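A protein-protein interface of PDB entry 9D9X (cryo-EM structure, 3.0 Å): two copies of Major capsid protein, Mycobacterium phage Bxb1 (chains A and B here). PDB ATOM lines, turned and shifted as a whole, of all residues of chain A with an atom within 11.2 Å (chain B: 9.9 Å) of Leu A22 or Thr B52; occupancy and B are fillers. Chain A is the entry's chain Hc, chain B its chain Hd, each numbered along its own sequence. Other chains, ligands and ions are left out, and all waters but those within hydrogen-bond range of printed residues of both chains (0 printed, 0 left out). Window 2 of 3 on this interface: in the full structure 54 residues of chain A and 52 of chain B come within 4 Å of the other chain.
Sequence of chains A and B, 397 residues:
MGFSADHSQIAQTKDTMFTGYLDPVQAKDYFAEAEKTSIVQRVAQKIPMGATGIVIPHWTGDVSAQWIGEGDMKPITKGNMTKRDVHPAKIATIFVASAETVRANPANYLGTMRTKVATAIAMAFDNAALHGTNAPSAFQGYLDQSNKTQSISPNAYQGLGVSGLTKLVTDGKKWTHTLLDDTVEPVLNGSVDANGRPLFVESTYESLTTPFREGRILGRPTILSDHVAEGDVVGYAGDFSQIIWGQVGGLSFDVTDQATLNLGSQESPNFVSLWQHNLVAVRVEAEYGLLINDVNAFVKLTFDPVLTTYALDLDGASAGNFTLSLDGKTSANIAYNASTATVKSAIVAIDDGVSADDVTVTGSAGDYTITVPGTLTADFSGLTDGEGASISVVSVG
O of Asp A23 lies within hydrogen-bond range of OG1 of Thr B52, at 2.9 Å. N of Val A25 is in hydrogen-bond range of O of Gly B53. The backbone NH of Val B55 lies within hydrogen-bond range of the backbone carbonyl oxygen of Val A25, at 2.8 Å. N of Ala A27 is in hydrogen-bond range of O of Val B55, at 2.9 Å.
The backbone carbonyl oxygen of Thr B52 lies within hydrogen-bond range of a ring nitrogen (ND1) of His B87, at 2.9 Å. The backbone carbonyl oxygen of Ile B54 lies within hydrogen-bond range of the backbone NH of Val B86.
CB of Thr B52 touches O of Leu A22, 3.7 Å away. Pro A24 touches Thr B52 (CA to OG1, 3.7 Å). Pro A24 touches Gly B53. Ile B54 touches Pro A24. CG of Pro A24 touches CG2 of Val B55, 3.5 Å away. Val A25 touches Ile B54 (O to CA, 3.3 Å). Val B55 touches Gln A26 (CG1 to OE1, 3.5 Å).
No residue of chain B comes within 4 Å of Thr A13. No residue of chain B comes within 4 Å of Gly A20. Tyr A21 touches none of the printed residues of chain B. Of the printed residues of chain B, Asp A23 touches Thr B52. Of the printed residues of chain B, Val A25 touches Gly B53, Ile B54 and Val B55. Printed residues of chain B within 4 Å of Gln A26: Val B55 (3.5 Å). Of the printed residues of chain B, Ala A27 touches Val B55 (2.9 Å). Pro B48 touches none of the printed residues of chain A. No residue of chain A comes within 4 Å of Gly B50. Ala B51 touches none of the printed residues of chain A. Thr B52 touches just these residues of chain A: Leu A22 (3.7 Å), Asp A23 (2.9 Å) and Pro A24 (3.7 Å). Of chain A, only Pro A24 and Val A25 come within 4 Å of Gly B53. Of the printed residues of chain A, Ile B54 touches Pro A24 and Val A25. Of the printed residues of chain A, Val B55 touches Pro A24, Val A25, Gln A26 and Ala A27. No residue of chain A comes within 4 Å of His B87. The nearest residue of chain A that does not touch Thr B52 is Val A25 (4.3 Å).
Printed residues of chain A that touch a printed residue of chain B: Leu A22, Asp A23, Pro A24, Val A25, Gln A26 and Ala A27. Among the printed residues, 11 pairs touch across the chains. Among the printed residues, no Asp or Glu carboxylate lies within 4 Å of a Lys or Arg side-chain nitrogen of the other chain.
No position is printed for both chains. Of the 11 pairs that touch across the chains among the printed residues, none has its exchanged pair printed and touching as well.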
ATOM      1  N   ALA A  11     -25.731 -28.420  14.291  1.00  0.00           N
ATOM      2  CA  ALA A  11     -24.930 -27.475  13.520  1.00  0.00           C
ATOM      3  C   ALA A  11     -25.655 -26.134  13.368  1.00  0.00           C
ATOM      4  O   ALA A  11     -26.774 -26.096  12.864  1.00  0.00           O
ATOM      5  CB  ALA A  11     -24.617 -28.094  12.161  1.00  0.00           C
ATOM      6  N   GLN A  12     -25.041 -25.033  13.787  1.00  0.00           N
ATOM      7  CA  GLN A  12     -25.622 -23.688  13.769  1.00  0.00           C
ATOM      8  C   GLN A  12     -24.691 -22.719  13.054  1.00  0.00           C
ATOM      9  O   GLN A  12     -23.475 -22.866  13.128  1.00  0.00           O
ATOM     10  CB  GLN A  12     -25.836 -23.161  15.189  1.00  0.00           C
ATOM     11  CG  GLN A  12     -26.588 -24.111  16.123  1.00  0.00           C
ATOM     12  CD  GLN A  12     -26.379 -23.735  17.578  1.00  0.00           C
ATOM     13  OE1 GLN A  12     -27.302 -23.336  18.266  1.00  0.00           O
ATOM     14  NE2 GLN A  12     -25.171 -23.796  18.094  1.00  0.00           N
ATOM     15  N   THR A  13     -25.206 -21.664  12.426  1.00  0.00           N
ATOM     16  CA  THR A  13     -24.326 -20.718  11.723  1.00  0.00           C
ATOM     17  C   THR A  13     -23.362 -19.979  12.651  1.00  0.00           C
ATOM     18  O   THR A  13     -22.317 -19.518  12.202  1.00  0.00           O
ATOM     19  CB  THR A  13     -25.106 -19.697  10.908  1.00  0.00           C
ATOM     20  OG1 THR A  13     -25.785 -18.801  11.741  1.00  0.00           O
ATOM     21  CG2 THR A  13     -26.097 -20.327   9.941  1.00  0.00           C
ATOM     22  N   LYS A  14     -23.666 -19.892  13.949  1.00  0.00           N
ATOM     23  CA  LYS A  14     -22.792 -19.312  14.971  1.00  0.00           C
ATOM     24  C   LYS A  14     -21.665 -20.229  15.459  1.00  0.00           C
ATOM     25  O   LYS A  14     -20.796 -19.755  16.187  1.00  0.00           O
ATOM     26  CB  LYS A  14     -23.639 -18.774  16.133  1.00  0.00           C
ATOM     27  CG  LYS A  14     -24.393 -19.853  16.919  1.00  0.00           C
ATOM     28  CD  LYS A  14     -25.198 -19.251  18.075  1.00  0.00           C
ATOM     29  CE  LYS A  14     -25.871 -20.363  18.882  1.00  0.00           C
ATOM     30  NZ  LYS A  14     -26.672 -19.823  20.013  1.00  0.00           N
ATOM     31  N   ASP A  15     -21.642 -21.508  15.088  1.00  0.00           N
ATOM     32  CA  ASP A  15     -20.566 -22.422  15.496  1.00  0.00           C
ATOM     33  C   ASP A  15     -19.213 -21.986  14.920  1.00  0.00           C
ATOM     34  O   ASP A  15     -19.123 -21.468  13.806  1.00  0.00           O
ATOM     35  CB  ASP A  15     -20.823 -23.867  15.050  1.00  0.00           C
ATOM     36  CG  ASP A  15     -22.103 -24.544  15.555  1.00  0.00           C
ATOM     37  OD1 ASP A  15     -22.684 -24.140  16.585  1.00  0.00           O
ATOM     38  OD2 ASP A  15     -22.496 -25.540  14.910  1.00  0.00           O
ATOM     39  N   THR A  16     -18.128 -22.252  15.640  1.00  0.00           N
ATOM     40  CA  THR A  16     -16.781 -21.810  15.249  1.00  0.00           C
ATOM     41  C   THR A  16     -16.313 -22.388  13.917  1.00  0.00           C
ATOM     42  O   THR A  16     -15.604 -21.709  13.175  1.00  0.00           O
ATOM     43  CB  THR A  16     -15.757 -22.157  16.328  1.00  0.00           C
ATOM     44  OG1 THR A  16     -15.781 -23.534  16.600  1.00  0.00           O
ATOM     45  CG2 THR A  16     -16.018 -21.419  17.635  1.00  0.00           C
ATOM     46  N   MET A  17     -16.763 -23.589  13.553  1.00  0.00           N
ATOM     47  CA  MET A  17     -16.372 -24.267  12.316  1.00  0.00           C
ATOM     48  C   MET A  17     -16.751 -23.515  11.034  1.00  0.00           C
ATOM     49  O   MET A  17     -16.230 -23.842   9.974  1.00  0.00           O
ATOM     50  CB  MET A  17     -16.946 -25.692  12.297  1.00  0.00           C
ATOM     51  CG  MET A  17     -18.435 -25.767  11.943  1.00  0.00           C
ATOM     52  SD  MET A  17     -19.091 -27.440  11.747  1.00  0.00           S
ATOM     53  CE  MET A  17     -19.119 -27.974  13.472  1.00  0.00           C
ATOM     54  N   PHE A  18     -17.651 -22.532  11.100  1.00  0.00           N
ATOM     55  CA  PHE A  18     -18.074 -21.737   9.948  1.00  0.00           C
ATOM     56  C   PHE A  18     -17.385 -20.375   9.861  1.00  0.00           C
ATOM     57  O   PHE A  18     -17.619 -19.642   8.907  1.00  0.00           O
ATOM     58  CB  PHE A  18     -19.592 -21.567   9.966  1.00  0.00           C
ATOM     59  CG  PHE A  18     -20.341 -22.873   9.895  1.00  0.00           C
ATOM     60  CD1 PHE A  18     -20.451 -23.549   8.672  1.00  0.00           C
ATOM     61  CD2 PHE A  18     -20.918 -23.416  11.049  1.00  0.00           C
ATOM     62  CE1 PHE A  18     -21.129 -24.775   8.607  1.00  0.00           C
ATOM     63  CE2 PHE A  18     -21.599 -24.641  10.986  1.00  0.00           C
ATOM     64  CZ  PHE A  18     -21.703 -25.321   9.764  1.00  0.00           C
ATOM     65  N   THR A  19     -16.539 -20.004  10.821  1.00  0.00           N
ATOM     66  CA  THR A  19     -15.799 -18.735  10.757  1.00  0.00           C
ATOM     67  C   THR A  19     -14.996 -18.637   9.460  1.00  0.00           C
ATOM     68  O   THR A  19     -14.394 -19.606   9.007  1.00  0.00           O
ATOM     69  CB  THR A  19     -14.889 -18.531  11.972  1.00  0.00           C
ATOM     70  OG1 THR A  19     -14.048 -19.635  12.202  1.00  0.00           O
ATOM     71  CG2 THR A  19     -15.688 -18.298  13.249  1.00  0.00           C
ATOM     72  N   GLY A  20     -15.028 -17.477   8.811  1.00  0.00           N
ATOM     73  CA  GLY A  20     -14.446 -17.266   7.481  1.00  0.00           C
ATOM     74  C   GLY A  20     -15.364 -17.632   6.312  1.00  0.00           C
ATOM     75  O   GLY A  20     -15.100 -17.242   5.177  1.00  0.00           O
ATOM     76  N   TYR A  21     -16.462 -18.329   6.567  1.00  0.00           N
ATOM     77  CA  TYR A  21     -17.616 -18.402   5.677  1.00  0.00           C
ATOM     78  C   TYR A  21     -18.707 -17.474   6.208  1.00  0.00           C
ATOM     79  O   TYR A  21     -18.609 -16.962   7.324  1.00  0.00           O
ATOM     80  CB  TYR A  21     -18.101 -19.848   5.573  1.00  0.00           C
ATOM     81  CG  TYR A  21     -17.013 -20.810   5.161  1.00  0.00           C
ATOM     82  CD1 TYR A  21     -16.752 -21.024   3.800  1.00  0.00           C
ATOM     83  CD2 TYR A  21     -16.232 -21.451   6.138  1.00  0.00           C
ATOM     84  CE1 TYR A  21     -15.707 -21.877   3.413  1.00  0.00           C
ATOM     85  CE2 TYR A  21     -15.186 -22.305   5.755  1.00  0.00           C
ATOM     86  CZ  TYR A  21     -14.922 -22.517   4.390  1.00  0.00           C
ATOM     87  OH  TYR A  21     -13.907 -23.332   4.013  1.00  0.00           O
ATOM     88  N   LEU A  22     -19.769 -17.252   5.436  1.00  0.00           N
ATOM     89  CA  LEU A  22     -20.885 -16.402   5.865  1.00  0.00           C
ATOM     90  C   LEU A  22     -20.453 -14.957   6.193  1.00  0.00           C
ATOM     91  O   LEU A  22     -20.945 -14.348   7.140  1.00  0.00           O
ATOM     92  CB  LEU A  22     -21.676 -17.060   7.021  1.00  0.00           C
ATOM     93  CG  LEU A  22     -22.020 -18.542   6.841  1.00  0.00           C
ATOM     94  CD1 LEU A  22     -22.794 -19.026   8.058  1.00  0.00           C
ATOM     95  CD2 LEU A  22     -22.874 -18.790   5.602  1.00  0.00           C
ATOM     96  N   ASP A  23     -19.524 -14.396   5.421  1.00  0.00           N
ATOM     97  CA  ASP A  23     -19.093 -13.003   5.571  1.00  0.00           C
ATOM     98  C   ASP A  23     -20.149 -11.998   5.076  1.00  0.00           C
ATOM     99  O   ASP A  23     -20.897 -12.292   4.138  1.00  0.00           O
ATOM    100  CB  ASP A  23     -17.770 -12.767   4.828  1.00  0.00           C
ATOM    101  CG  ASP A  23     -16.534 -13.287   5.570  1.00  0.00           C
ATOM    102  OD1 ASP A  23     -16.583 -13.448   6.811  1.00  0.00           O
ATOM    103  OD2 ASP A  23     -15.485 -13.471   4.911  1.00  0.00           O
ATOM    104  N   PRO A  24     -20.218 -10.795   5.668  1.00  0.00           N
ATOM    105  CA  PRO A  24     -21.129  -9.744   5.246  1.00  0.00           C
ATOM    106  C   PRO A  24     -20.747  -9.132   3.898  1.00  0.00           C
ATOM    107  O   PRO A  24     -19.583  -9.114   3.510  1.00  0.00           O
ATOM    108  CB  PRO A  24     -21.092  -8.711   6.367  1.00  0.00           C
ATOM    109  CG  PRO A  24     -19.705  -8.887   6.965  1.00  0.00           C
ATOM    110  CD  PRO A  24     -19.468 -10.380   6.838  1.00  0.00           C
ATOM    111  N   VAL A  25     -21.732  -8.602   3.181  1.00  0.00           N
ATOM    112  CA  VAL A  25     -21.549  -7.949   1.879  1.00  0.00           C
ATOM    113  C   VAL A  25     -21.053  -6.511   2.043  1.00  0.00           C
ATOM    114  O   VAL A  25     -21.437  -5.819   2.980  1.00  0.00           O
ATOM    115  CB  VAL A  25     -22.863  -8.001   1.089  1.00  0.00           C
ATOM    116  CG1 VAL A  25     -22.740  -7.373  -0.302  1.00  0.00           C
ATOM    117  CG2 VAL A  25     -23.323  -9.447   0.893  1.00  0.00           C
ATOM    118  N   GLN A  26     -20.212  -6.021   1.137  1.00  0.00           N
ATOM    119  CA  GLN A  26     -19.729  -4.639   1.161  1.00  0.00           C
ATOM    120  C   GLN A  26     -20.789  -3.663   0.630  1.00  0.00           C
ATOM    121  O   GLN A  26     -21.155  -3.734  -0.544  1.00  0.00           O
ATOM    122  CB  GLN A  26     -18.442  -4.572   0.330  1.00  0.00           C
ATOM    123  CG  GLN A  26     -17.732  -3.214   0.425  1.00  0.00           C
ATOM    124  CD  GLN A  26     -17.088  -2.961   1.781  1.00  0.00           C
ATOM    125  OE1 GLN A  26     -16.967  -3.833   2.628  1.00  0.00           O
ATOM    126  NE2 GLN A  26     -16.631  -1.758   2.041  1.00  0.00           N
ATOM    127  N   ALA A  27     -21.266  -2.735   1.456  1.00  0.00           N
ATOM    128  CA  ALA A  27     -22.225  -1.702   1.068  1.00  0.00           C
ATOM    129  C   ALA A  27     -21.547  -0.349   0.787  1.00  0.00           C
ATOM    130  O   ALA A  27     -20.403  -0.120   1.178  1.00  0.00           O
ATOM    131  CB  ALA A  27     -23.274  -1.592   2.176  1.00  0.00           C
ATOM    132  N   PRO B  48     -30.997  -2.712   0.541  1.00  0.00           N
ATOM    133  CA  PRO B  48     -30.822  -4.134   0.286  1.00  0.00           C
ATOM    134  C   PRO B  48     -30.040  -4.810   1.405  1.00  0.00           C
ATOM    135  O   PRO B  48     -29.039  -4.271   1.870  1.00  0.00           O
ATOM    136  CB  PRO B  48     -30.072  -4.244  -1.036  1.00  0.00           C
ATOM    137  CG  PRO B  48     -30.336  -2.907  -1.713  1.00  0.00           C
ATOM    138  CD  PRO B  48     -30.435  -1.938  -0.544  1.00  0.00           C
ATOM    139  N   MET B  49     -30.452  -6.006   1.819  1.00  0.00           N
ATOM    140  CA  MET B  49     -29.769  -6.749   2.876  1.00  0.00           C
ATOM    141  C   MET B  49     -29.957  -8.253   2.711  1.00  0.00           C
ATOM    142  O   MET B  49     -31.082  -8.748   2.710  1.00  0.00           O
ATOM    143  CB  MET B  49     -30.268  -6.263   4.238  1.00  0.00           C
ATOM    144  CG  MET B  49     -29.464  -6.891   5.372  1.00  0.00           C
ATOM    145  SD  MET B  49     -29.949  -6.319   7.010  1.00  0.00           S
ATOM    146  CE  MET B  49     -29.343  -4.615   6.995  1.00  0.00           C
ATOM    147  N   GLY B  50     -28.853  -8.982   2.570  1.00  0.00           N
ATOM    148  CA  GLY B  50     -28.826 -10.443   2.516  1.00  0.00           C
ATOM    149  C   GLY B  50     -28.655 -11.083   3.891  1.00  0.00           C
ATOM    150  O   GLY B  50     -28.388 -10.408   4.882  1.00  0.00           O
ATOM    151  N   ALA B  51     -28.768 -12.403   3.956  1.00  0.00           N
ATOM    152  CA  ALA B  51     -28.801 -13.146   5.211  1.00  0.00           C
ATOM    153  C   ALA B  51     -27.535 -13.004   6.067  1.00  0.00           C
ATOM    154  O   ALA B  51     -27.607 -13.062   7.292  1.00  0.00           O
ATOM    155  CB  ALA B  51     -29.048 -14.612   4.856  1.00  0.00           C
ATOM    156  N   THR B  52     -26.368 -12.799   5.456  1.00  0.00           N
ATOM    157  CA  THR B  52     -25.110 -12.620   6.197  1.00  0.00           C
ATOM    158  C   THR B  52     -24.927 -11.207   6.745  1.00  0.00           C
ATOM    159  O   THR B  52     -24.076 -10.987   7.603  1.00  0.00           O
ATOM    160  CB  THR B  52     -23.895 -13.004   5.354  1.00  0.00           C
ATOM    161  OG1 THR B  52     -23.782 -12.177   4.230  1.00  0.00           O
ATOM    162  CG2 THR B  52     -23.961 -14.443   4.856  1.00  0.00           C
ATOM    163  N   GLY B  53     -25.742 -10.244   6.315  1.00  0.00           N
ATOM    164  CA  GLY B  53     -25.633  -8.839   6.701  1.00  0.00           C
ATOM    165  C   GLY B  53     -24.766  -8.012   5.758  1.00  0.00           C
ATOM    166  O   GLY B  53     -24.464  -8.424   4.640  1.00  0.00           O
ATOM    167  N   ILE B  54     -24.359  -6.833   6.220  1.00  0.00           N
ATOM    168  CA  ILE B  54     -23.610  -5.838   5.443  1.00  0.00           C
ATOM    169  C   ILE B  54     -22.507  -5.182   6.262  1.00  0.00           C
ATOM    170  O   ILE B  54     -22.597  -5.108   7.485  1.00  0.00           O
ATOM    171  CB  ILE B  54     -24.539  -4.753   4.874  1.00  0.00           C
ATOM    172  CG1 ILE B  54     -25.277  -3.991   5.994  1.00  0.00           C
ATOM    173  CG2 ILE B  54     -25.496  -5.356   3.844  1.00  0.00           C
ATOM    174  CD1 ILE B  54     -26.180  -2.868   5.491  1.00  0.00           C
ATOM    175  N   VAL B  55     -21.484  -4.676   5.580  1.00  0.00           N
ATOM    176  CA  VAL B  55     -20.427  -3.805   6.116  1.00  0.00           C
ATOM    177  C   VAL B  55     -20.505  -2.443   5.452  1.00  0.00           C
ATOM    178  O   VAL B  55     -20.615  -2.358   4.231  1.00  0.00           O
ATOM    179  CB  VAL B  55     -19.043  -4.434   5.921  1.00  0.00           C
ATOM    180  CG1 VAL B  55     -17.880  -3.445   6.020  1.00  0.00           C
ATOM    181  CG2 VAL B  55     -18.809  -5.473   7.011  1.00  0.00           C
ATOM    182  N   ARG B  84     -18.289  -0.428   9.997  1.00  0.00           N
ATOM    183  CA  ARG B  84     -19.293  -1.017  10.899  1.00  0.00           C
ATOM    184  C   ARG B  84     -20.048  -2.137  10.183  1.00  0.00           C
ATOM    185  O   ARG B  84     -20.327  -2.005   8.997  1.00  0.00           O
ATOM    186  CB  ARG B  84     -20.237   0.105  11.350  1.00  0.00           C
ATOM    187  CG  ARG B  84     -21.279  -0.360  12.370  1.00  0.00           C
ATOM    188  CD  ARG B  84     -22.420   0.647  12.502  1.00  0.00           C
ATOM    189  NE  ARG B  84     -22.042   1.841  13.269  1.00  0.00           N
ATOM    190  CZ  ARG B  84     -22.335   2.080  14.529  1.00  0.00           C
ATOM    191  NH1 ARG B  84     -22.058   3.235  15.054  1.00  0.00           N
ATOM    192  NH2 ARG B  84     -22.903   1.202  15.302  1.00  0.00           N
ATOM    193  N   ASP B  85     -20.401  -3.216  10.876  1.00  0.00           N
ATOM    194  CA  ASP B  85     -21.174  -4.336  10.331  1.00  0.00           C
ATOM    195  C   ASP B  85     -22.558  -4.467  10.980  1.00  0.00           C
ATOM    196  O   ASP B  85     -22.737  -4.157  12.156  1.00  0.00           O
ATOM    197  CB  ASP B  85     -20.409  -5.658  10.459  1.00  0.00           C
ATOM    198  CG  ASP B  85     -20.185  -6.119  11.903  1.00  0.00           C
ATOM    199  OD1 ASP B  85     -19.773  -5.296  12.752  1.00  0.00           O
ATOM    200  OD2 ASP B  85     -20.385  -7.328  12.173  1.00  0.00           O
ATOM    201  N   VAL B  86     -23.550  -4.934  10.219  1.00  0.00           N
ATOM    202  CA  VAL B  86     -24.952  -5.074  10.646  1.00  0.00           C
ATOM    203  C   VAL B  86     -25.523  -6.417  10.184  1.00  0.00           C
ATOM    204  O   VAL B  86     -25.393  -6.743   9.005  1.00  0.00           O
ATOM    205  CB  VAL B  86     -25.797  -3.924  10.067  1.00  0.00           C
ATOM    206  CG1 VAL B  86     -27.253  -3.979  10.537  1.00  0.00           C
ATOM    207  CG2 VAL B  86     -25.253  -2.547  10.446  1.00  0.00           C
ATOM    208  N   HIS B  87     -26.195  -7.174  11.061  1.00  0.00           N
ATOM    209  CA  HIS B  87     -26.791  -8.489  10.757  1.00  0.00           C
ATOM    210  C   HIS B  87     -28.301  -8.522  11.056  1.00  0.00           C
ATOM    211  O   HIS B  87     -28.723  -7.885  12.018  1.00  0.00           O
ATOM    212  CB  HIS B  87     -26.079  -9.594  11.553  1.00  0.00           C
ATOM    213  CG  HIS B  87     -24.583  -9.592  11.397  1.00  0.00           C
ATOM    214  ND1 HIS B  87     -23.863 -10.014  10.294  1.00  0.00           N
ATOM    215  CD2 HIS B  87     -23.704  -9.025  12.273  1.00  0.00           C
ATOM    216  CE1 HIS B  87     -22.573  -9.700  10.498  1.00  0.00           C
ATOM    217  NE2 HIS B  87     -22.453  -9.096  11.695  1.00  0.00           N
ATOM    218  N   PRO B  88     -29.129  -9.249  10.293  1.00  0.00           N
ATOM    219  CA  PRO B  88     -30.549  -9.413  10.588  1.00  0.00           C
ATOM    220  C   PRO B  88     -30.864 -10.117  11.915  1.00  0.00           C
ATOM    221  O   PRO B  88     -30.014 -10.772  12.513  1.00  0.00           O
ATOM    222  CB  PRO B  88     -31.126 -10.227   9.435  1.00  0.00           C
ATOM    223  CG  PRO B  88     -30.137 -10.012   8.305  1.00  0.00           C
ATOM    224  CD  PRO B  88     -28.807  -9.865   9.023  1.00  0.00           C
ATOM    225  N   ALA B  89     -32.130 -10.049  12.312  1.00  0.00           N
ATOM    226  CA  ALA B  89     -32.758 -10.807  13.384  1.00  0.00           C
ATOM    227  C   ALA B  89     -34.118 -11.355  12.930  1.00  0.00           C
ATOM    228  O   ALA B  89     -34.733 -10.845  11.994  1.00  0.00           O
ATOM    229  CB  ALA B  89     -32.908  -9.913  14.610  1.00  0.00           C
ATOM    230  N   ALA B 138     -28.986  -7.981  17.831  1.00  0.00           N
ATOM    231  CA  ALA B 138     -28.483  -7.632  16.513  1.00  0.00           C
ATOM    232  C   ALA B 138     -28.975  -6.279  15.982  1.00  0.00           C
ATOM    233  O   ALA B 138     -28.399  -5.764  15.030  1.00  0.00           O
ATOM    234  CB  ALA B 138     -28.857  -8.761  15.560  1.00  0.00           C
ATOM    235  N   VAL B 248     -35.113  -9.360   5.005  1.00  0.00           N
ATOM    236  CA  VAL B 248     -34.656 -10.528   4.253  1.00  0.00           C
ATOM    237  C   VAL B 248     -35.876 -11.305   3.778  1.00  0.00           C
ATOM    238  O   VAL B 248     -36.672 -11.767   4.589  1.00  0.00           O
ATOM    239  CB  VAL B 248     -33.750 -11.419   5.112  1.00  0.00           C
ATOM    240  CG1 VAL B 248     -33.125 -12.519   4.254  1.00  0.00           C
ATOM    241  CG2 VAL B 248     -32.615 -10.640   5.772  1.00  0.00           C
ATOM    242  N   GLU B 287     -37.998 -11.591   8.936  1.00  0.00           N
ATOM    243  CA  GLU B 287     -36.595 -11.324   9.263  1.00  0.00           C
ATOM    244  C   GLU B 287     -36.151  -9.916   8.840  1.00  0.00           C
ATOM    245  O   GLU B 287     -36.345  -9.520   7.695  1.00  0.00           O
ATOM    246  CB  GLU B 287     -35.781 -12.443   8.615  1.00  0.00           C
ATOM    247  CG  GLU B 287     -34.320 -12.507   9.053  1.00  0.00           C
ATOM    248  CD  GLU B 287     -33.651 -13.830   8.641  1.00  0.00           C
ATOM    249  OE1 GLU B 287     -34.341 -14.873   8.528  1.00  0.00           O
ATOM    250  OE2 GLU B 287     -32.412 -13.843   8.468  1.00  0.00           O
